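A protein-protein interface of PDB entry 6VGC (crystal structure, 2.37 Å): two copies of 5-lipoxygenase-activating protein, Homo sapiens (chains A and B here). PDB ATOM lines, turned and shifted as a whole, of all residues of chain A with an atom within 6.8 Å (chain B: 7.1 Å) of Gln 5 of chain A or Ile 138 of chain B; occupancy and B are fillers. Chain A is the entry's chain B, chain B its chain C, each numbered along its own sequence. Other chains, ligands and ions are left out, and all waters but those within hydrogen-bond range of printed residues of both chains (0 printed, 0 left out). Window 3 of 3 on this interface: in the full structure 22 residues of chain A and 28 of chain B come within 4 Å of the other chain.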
ATOM      1  N   LEU A   3     -12.212   8.278 -23.923  1.00  0.00           N
ATOM      2  CA  LEU A   3     -12.642   9.130 -25.035  1.00  0.00           C
ATOM      3  C   LEU A   3     -11.468   9.674 -25.845  1.00  0.00           C
ATOM      4  O   LEU A   3     -10.377   9.888 -25.311  1.00  0.00           O
ATOM      5  CB  LEU A   3     -13.511  10.289 -24.530  1.00  0.00           C
ATOM      6  CG  LEU A   3     -14.906   9.992 -23.969  1.00  0.00           C
ATOM      7  CD1 LEU A   3     -15.517  11.261 -23.394  1.00  0.00           C
ATOM      8  CD2 LEU A   3     -15.830   9.386 -25.022  1.00  0.00           C
ATOM      9  N   ASP A   4     -11.709   9.894 -27.136  1.00  0.00           N
ATOM     10  CA  ASP A   4     -10.687  10.393 -28.055  1.00  0.00           C
ATOM     11  C   ASP A   4     -10.429  11.890 -27.880  1.00  0.00           C
ATOM     12  O   ASP A   4     -11.292  12.627 -27.397  1.00  0.00           O
ATOM     13  CB  ASP A   4     -11.064  10.067 -29.507  1.00  0.00           C
ATOM     14  CG  ASP A   4     -12.420  10.625 -29.903  1.00  0.00           C
ATOM     15  OD1 ASP A   4     -13.415   9.870 -29.841  1.00  0.00           O
ATOM     16  OD2 ASP A   4     -12.495  11.817 -30.267  1.00  0.00           O
ATOM     17  N   GLN A   5      -9.235  12.321 -28.290  1.00  0.00           N
ATOM     18  CA  GLN A   5      -8.751  13.696 -28.120  1.00  0.00           C
ATOM     19  C   GLN A   5      -9.714  14.768 -28.641  1.00  0.00           C
ATOM     20  O   GLN A   5      -9.862  15.827 -28.025  1.00  0.00           O
ATOM     21  CB  GLN A   5      -7.381  13.848 -28.794  1.00  0.00           C
ATOM     22  CG  GLN A   5      -6.578  15.075 -28.368  1.00  0.00           C
ATOM     23  CD  GLN A   5      -5.926  14.924 -27.000  1.00  0.00           C
ATOM     24  OE1 GLN A   5      -5.864  13.829 -26.437  1.00  0.00           O
ATOM     25  NE2 GLN A   5      -5.427  16.030 -26.464  1.00  0.00           N
ATOM     26  N   GLU A   6     -10.356  14.486 -29.772  1.00  0.00           N
ATOM     27  CA  GLU A   6     -11.291  15.418 -30.406  1.00  0.00           C
ATOM     28  C   GLU A   6     -12.550  15.621 -29.563  1.00  0.00           C
ATOM     29  O   GLU A   6     -13.038  16.746 -29.428  1.00  0.00           O
ATOM     30  CB  GLU A   6     -11.677  14.933 -31.810  1.00  0.00           C
ATOM     31  CG  GLU A   6     -10.521  14.858 -32.813  1.00  0.00           C
ATOM     32  CD  GLU A   6      -9.614  13.650 -32.602  1.00  0.00           C
ATOM     33  OE1 GLU A   6     -10.102  12.601 -32.128  1.00  0.00           O
ATOM     34  OE2 GLU A   6      -8.409  13.753 -32.915  1.00  0.00           O
ATOM     35  N   THR A   7     -13.064  14.528 -29.000  1.00  0.00           N
ATOM     36  CA  THR A   7     -14.279  14.562 -28.190  1.00  0.00           C
ATOM     37  C   THR A   7     -14.042  15.282 -26.862  1.00  0.00           C
ATOM     38  O   THR A   7     -14.847  16.125 -26.460  1.00  0.00           O
ATOM     39  CB  THR A   7     -14.841  13.143 -27.940  1.00  0.00           C
ATOM     40  OG1 THR A   7     -14.902  12.426 -29.179  1.00  0.00           O
ATOM     41  CG2 THR A   7     -16.239  13.206 -27.333  1.00  0.00           C
ATOM     42  N   VAL A   8     -12.932  14.958 -26.195  1.00  0.00           N
ATOM     43  CA  VAL A   8     -12.567  15.606 -24.932  1.00  0.00           C
ATOM     44  C   VAL A   8     -12.467  17.123 -25.113  1.00  0.00           C
ATOM     45  O   VAL A   8     -12.918  17.884 -24.260  1.00  0.00           O
ATOM     46  CB  VAL A   8     -11.253  15.035 -24.328  1.00  0.00           C
ATOM     47  CG1 VAL A   8     -10.943  15.694 -22.988  1.00  0.00           C
ATOM     48  CG2 VAL A   8     -11.350  13.527 -24.154  1.00  0.00           C
ATOM     49  N   GLY A   9     -11.894  17.547 -26.239  1.00  0.00           N
ATOM     50  CA  GLY A   9     -11.784  18.965 -26.583  1.00  0.00           C
ATOM     51  C   GLY A   9     -13.116  19.688 -26.680  1.00  0.00           C
ATOM     52  O   GLY A   9     -13.194  20.886 -26.416  1.00  0.00           O
ATOM     53  N   ASN A  10     -14.161  18.954 -27.056  1.00  0.00           N
ATOM     54  CA  ASN A  10     -15.520  19.492 -27.126  1.00  0.00           C
ATOM     55  C   ASN A  10     -16.262  19.464 -25.788  1.00  0.00           C
ATOM     56  O   ASN A  10     -17.371  19.993 -25.686  1.00  0.00           O
ATOM     57  CB  ASN A  10     -16.339  18.734 -28.178  1.00  0.00           C
ATOM     58  CG  ASN A  10     -15.862  18.989 -29.597  1.00  0.00           C
ATOM     59  OD1 ASN A  10     -15.570  18.050 -30.340  1.00  0.00           O
ATOM     60  ND2 ASN A  10     -15.785  20.259 -29.982  1.00  0.00           N
ATOM     61  N   GLY B 131      -6.993  13.288 -15.567  1.00  0.00           N
ATOM     62  CA  GLY B 131      -7.466  13.070 -16.930  1.00  0.00           C
ATOM     63  C   GLY B 131      -7.465  14.330 -17.776  1.00  0.00           C
ATOM     64  O   GLY B 131      -7.090  14.294 -18.951  1.00  0.00           O
ATOM     65  N   PHE B 133      -5.579  17.073 -17.181  1.00  0.00           N
ATOM     66  CA  PHE B 133      -4.160  17.383 -17.376  1.00  0.00           C
ATOM     67  C   PHE B 133      -3.550  16.533 -18.487  1.00  0.00           C
ATOM     68  O   PHE B 133      -2.731  17.020 -19.269  1.00  0.00           O
ATOM     69  CB  PHE B 133      -3.363  17.199 -16.077  1.00  0.00           C
ATOM     70  CG  PHE B 133      -3.313  18.430 -15.211  1.00  0.00           C
ATOM     71  CD1 PHE B 133      -2.628  19.567 -15.632  1.00  0.00           C
ATOM     72  CD2 PHE B 133      -3.938  18.448 -13.969  1.00  0.00           C
ATOM     73  CE1 PHE B 133      -2.578  20.706 -14.835  1.00  0.00           C
ATOM     74  CE2 PHE B 133      -3.892  19.584 -13.163  1.00  0.00           C
ATOM     75  CZ  PHE B 133      -3.211  20.714 -13.597  1.00  0.00           C
ATOM     76  N   ASN B 134      -3.958  15.266 -18.548  1.00  0.00           N
ATOM     77  CA  ASN B 134      -3.503  14.344 -19.585  1.00  0.00           C
ATOM     78  C   ASN B 134      -3.913  14.808 -20.979  1.00  0.00           C
ATOM     79  O   ASN B 134      -3.092  14.810 -21.898  1.00  0.00           O
ATOM     80  CB  ASN B 134      -4.025  12.929 -19.316  1.00  0.00           C
ATOM     81  CG  ASN B 134      -3.548  11.922 -20.346  1.00  0.00           C
ATOM     82  OD1 ASN B 134      -4.327  11.457 -21.177  1.00  0.00           O
ATOM     83  ND2 ASN B 134      -2.262  11.586 -20.301  1.00  0.00           N
ATOM     84  N   TYR B 135      -5.179  15.202 -21.124  1.00  0.00           N
ATOM     85  CA  TYR B 135      -5.689  15.747 -22.380  1.00  0.00           C
ATOM     86  C   TYR B 135      -4.823  16.906 -22.876  1.00  0.00           C
ATOM     87  O   TYR B 135      -4.388  16.911 -24.028  1.00  0.00           O
ATOM     88  CB  TYR B 135      -7.157  16.191 -22.240  1.00  0.00           C
ATOM     89  CG  TYR B 135      -7.599  17.193 -23.291  1.00  0.00           C
ATOM     90  CD1 TYR B 135      -7.955  16.777 -24.575  1.00  0.00           C
ATOM     91  CD2 TYR B 135      -7.647  18.559 -23.004  1.00  0.00           C
ATOM     92  CE1 TYR B 135      -8.349  17.694 -25.547  1.00  0.00           C
ATOM     93  CE2 TYR B 135      -8.040  19.484 -23.970  1.00  0.00           C
ATOM     94  CZ  TYR B 135      -8.390  19.044 -25.237  1.00  0.00           C
ATOM     95  OH  TYR B 135      -8.777  19.953 -26.194  1.00  0.00           O
ATOM     96  N   TYR B 136      -4.571  17.874 -21.996  1.00  0.00           N
ATOM     97  CA  TYR B 136      -3.816  19.075 -22.357  1.00  0.00           C
ATOM     98  C   TYR B 136      -2.356  18.797 -22.719  1.00  0.00           C
ATOM     99  O   TYR B 136      -1.794  19.474 -23.577  1.00  0.00           O
ATOM    100  CB  TYR B 136      -3.917  20.142 -21.261  1.00  0.00           C
ATOM    101  CG  TYR B 136      -5.220  20.916 -21.278  1.00  0.00           C
ATOM    102  CD1 TYR B 136      -5.537  21.760 -22.342  1.00  0.00           C
ATOM    103  CD2 TYR B 136      -6.130  20.812 -20.226  1.00  0.00           C
ATOM    104  CE1 TYR B 136      -6.732  22.476 -22.363  1.00  0.00           C
ATOM    105  CE2 TYR B 136      -7.327  21.525 -20.236  1.00  0.00           C
ATOM    106  CZ  TYR B 136      -7.620  22.354 -21.308  1.00  0.00           C
ATOM    107  OH  TYR B 136      -8.799  23.063 -21.328  1.00  0.00           O
ATOM    108  N   LEU B 137      -1.754  17.800 -22.071  1.00  0.00           N
ATOM    109  CA  LEU B 137      -0.397  17.375 -22.409  1.00  0.00           C
ATOM    110  C   LEU B 137      -0.321  16.829 -23.833  1.00  0.00           C
ATOM    111  O   LEU B 137       0.632  17.113 -24.556  1.00  0.00           O
ATOM    112  CB  LEU B 137       0.122  16.334 -21.409  1.00  0.00           C
ATOM    113  CG  LEU B 137       0.627  16.826 -20.049  1.00  0.00           C
ATOM    114  CD1 LEU B 137       0.764  15.657 -19.081  1.00  0.00           C
ATOM    115  CD2 LEU B 137       1.952  17.577 -20.173  1.00  0.00           C
ATOM    116  N   ILE B 138      -1.335  16.056 -24.224  1.00  0.00           N
ATOM    117  CA  ILE B 138      -1.421  15.488 -25.571  1.00  0.00           C
ATOM    118  C   ILE B 138      -1.787  16.558 -26.608  1.00  0.00           C
ATOM    119  O   ILE B 138      -1.275  16.539 -27.731  1.00  0.00           O
ATOM    120  CB  ILE B 138      -2.427  14.304 -25.633  1.00  0.00           C
ATOM    121  CG1 ILE B 138      -2.042  13.218 -24.621  1.00  0.00           C
ATOM    122  CG2 ILE B 138      -2.491  13.711 -27.044  1.00  0.00           C
ATOM    123  CD1 ILE B 138      -3.167  12.244 -24.283  1.00  0.00           C
ATOM    124  N   PHE B 139      -2.663  17.485 -26.222  1.00  0.00           N
ATOM    125  CA  PHE B 139      -3.094  18.567 -27.110  1.00  0.00           C
ATOM    126  C   PHE B 139      -1.946  19.513 -27.458  1.00  0.00           C
ATOM    127  O   PHE B 139      -1.738  19.835 -28.630  1.00  0.00           O
ATOM    128  CB  PHE B 139      -4.265  19.348 -26.501  1.00  0.00           C
ATOM    129  CG  PHE B 139      -4.770  20.467 -27.374  1.00  0.00           C
ATOM    130  CD1 PHE B 139      -5.633  20.206 -28.436  1.00  0.00           C
ATOM    131  CD2 PHE B 139      -4.386  21.785 -27.131  1.00  0.00           C
ATOM    132  CE1 PHE B 139      -6.106  21.240 -29.248  1.00  0.00           C
ATOM    133  CE2 PHE B 139      -4.852  22.828 -27.937  1.00  0.00           C
ATOM    134  CZ  PHE B 139      -5.714  22.553 -28.997  1.00  0.00           C
ATOM    135  N   PHE B 140      -1.212  19.955 -26.436  1.00  0.00           N
ATOM    136  CA  PHE B 140      -0.057  20.834 -26.628  1.00  0.00           C
ATOM    137  C   PHE B 140       1.086  20.122 -27.347  1.00  0.00           C
ATOM    138  O   PHE B 140       1.856  20.754 -28.067  1.00  0.00           O
ATOM    139  CB  PHE B 140       0.420  21.427 -25.295  1.00  0.00           C
ATOM    140  CG  PHE B 140      -0.374  22.625 -24.841  1.00  0.00           C
ATOM    141  CD1 PHE B 140      -0.153  23.879 -25.405  1.00  0.00           C
ATOM    142  CD2 PHE B 140      -1.338  22.502 -23.844  1.00  0.00           C
ATOM    143  CE1 PHE B 140      -0.885  24.991 -24.987  1.00  0.00           C
ATOM    144  CE2 PHE B 140      -2.075  23.607 -23.417  1.00  0.00           C
ATOM    145  CZ  PHE B 140      -1.847  24.854 -23.990  1.00  0.00           C
ATOM    146  N   PHE B 141       1.182  18.808 -27.150  1.00  0.00           N
ATOM    147  CA  PHE B 141       2.133  17.977 -27.885  1.00  0.00           C
ATOM    148  C   PHE B 141       1.742  17.889 -29.359  1.00  0.00           C
ATOM    149  O   PHE B 141       2.604  17.923 -30.236  1.00  0.00           O
ATOM    150  CB  PHE B 141       2.202  16.573 -27.271  1.00  0.00           C
ATOM    151  CG  PHE B 141       3.372  15.755 -27.744  1.00  0.00           C
ATOM    152  CD1 PHE B 141       3.258  14.930 -28.860  1.00  0.00           C
ATOM    153  CD2 PHE B 141       4.586  15.795 -27.061  1.00  0.00           C
ATOM    154  CE1 PHE B 141       4.339  14.166 -29.298  1.00  0.00           C
ATOM    155  CE2 PHE B 141       5.674  15.033 -27.491  1.00  0.00           C
ATOM    156  CZ  PHE B 141       5.549  14.217 -28.612  1.00  0.00           C
ATOM    157  N   GLY B 142       0.440  17.782 -29.619  1.00  0.00           N
ATOM    158  CA  GLY B 142      -0.090  17.702 -30.980  1.00  0.00           C
ATOM    159  C   GLY B 142       0.069  18.982 -31.779  1.00  0.00           C
ATOM    160  O   GLY B 142       0.360  18.940 -32.976  1.00  0.00           O
ATOM    161  N   SER B 143      -0.128  20.121 -31.117  1.00  0.00           N
ATOM    162  CA  SER B 143       0.022  21.429 -31.757  1.00  0.00           C
ATOM    163  C   SER B 143       1.492  21.825 -31.905  1.00  0.00           C
ATOM    164  O   SER B 143       1.843  22.600 -32.800  1.00  0.00           O
ATOM    165  CB  SER B 143      -0.753  22.504 -30.989  1.00  0.00           C
ATOM    166  OG  SER B 143      -0.268  22.643 -29.666  1.00  0.00           O
ATOM    167  N   ASP B 144       2.340  21.294 -31.025  1.00  0.00           N
ATOM    168  CA  ASP B 144       3.785  21.507 -31.099  1.00  0.00           C
ATOM    169  C   ASP B 144       4.370  20.714 -32.265  1.00  0.00           C
ATOM    170  O   ASP B 144       5.306  21.166 -32.927  1.00  0.00           O
ATOM    171  CB  ASP B 144       4.459  21.088 -29.788  1.00  0.00           C
ATOM    172  CG  ASP B 144       5.701  21.905 -29.473  1.00  0.00           C
ATOM    173  OD1 ASP B 144       6.586  22.038 -30.347  1.00  0.00           O
ATOM    174  OD2 ASP B 144       5.797  22.408 -28.335  1.00  0.00           O
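Hydrophobic or aromatic side chains of chain B within 4 Å of the printed part of chain A: Tyr 135, Ile 138 and Phe 139.
Among the printed residues, merely in contact across the chains: Gln 5 of chain A with Ile 138 of chain B (3.4 Å), Val 8 of chain A with Tyr 135 of chain B (3.6 Å) and Gly 9 of chain A with Tyr 135 of chain B (3.2 Å).
The side-chain amide nitrogen (NE2) of Gln 5 of chain A lies within hydrogen-bond range of the backbone carbonyl oxygen (O) of Tyr 135 of chain B (2.8 Å). The backbone NH of Phe 139 of chain B sits close to the side-chain amide nitrogen of Gln 5 of chain A, 3.1 Å away.
O of Phe 139 of chain B sits at hydrogen-bond distance from OG of Ser 143 of chain B.
Of the printed residues of chain B, Val 8 of chain A touches Tyr 135. Printed residues of chain B within 4 Å of Gly 9 of chain A: Tyr 135 (3.2 Å). Phe 133 of chain B touches none of the printed residues of chain A. Printed residues of chain A within 4 Å of Tyr 135 of chain B: Gln 5 (2.8 Å), Val 8 (3.6 Å) and Gly 9 (3.2 Å). Ile 138 of chain B touches one residue of chain A. Printed residues of chain A within 4 Å of Phe 139 of chain B: Gln 5. Phe 141 of chain B touches none of the printed residues of chain A. The nearest printed residue of chain A that does not touch Ile 138 of chain B is Leu 3 of chain A (7.7 Å).
No position is printed for both chains. Of the 5 pairs that touch across the chains among the printed residues, none has its exchanged pair printed and touching as well.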
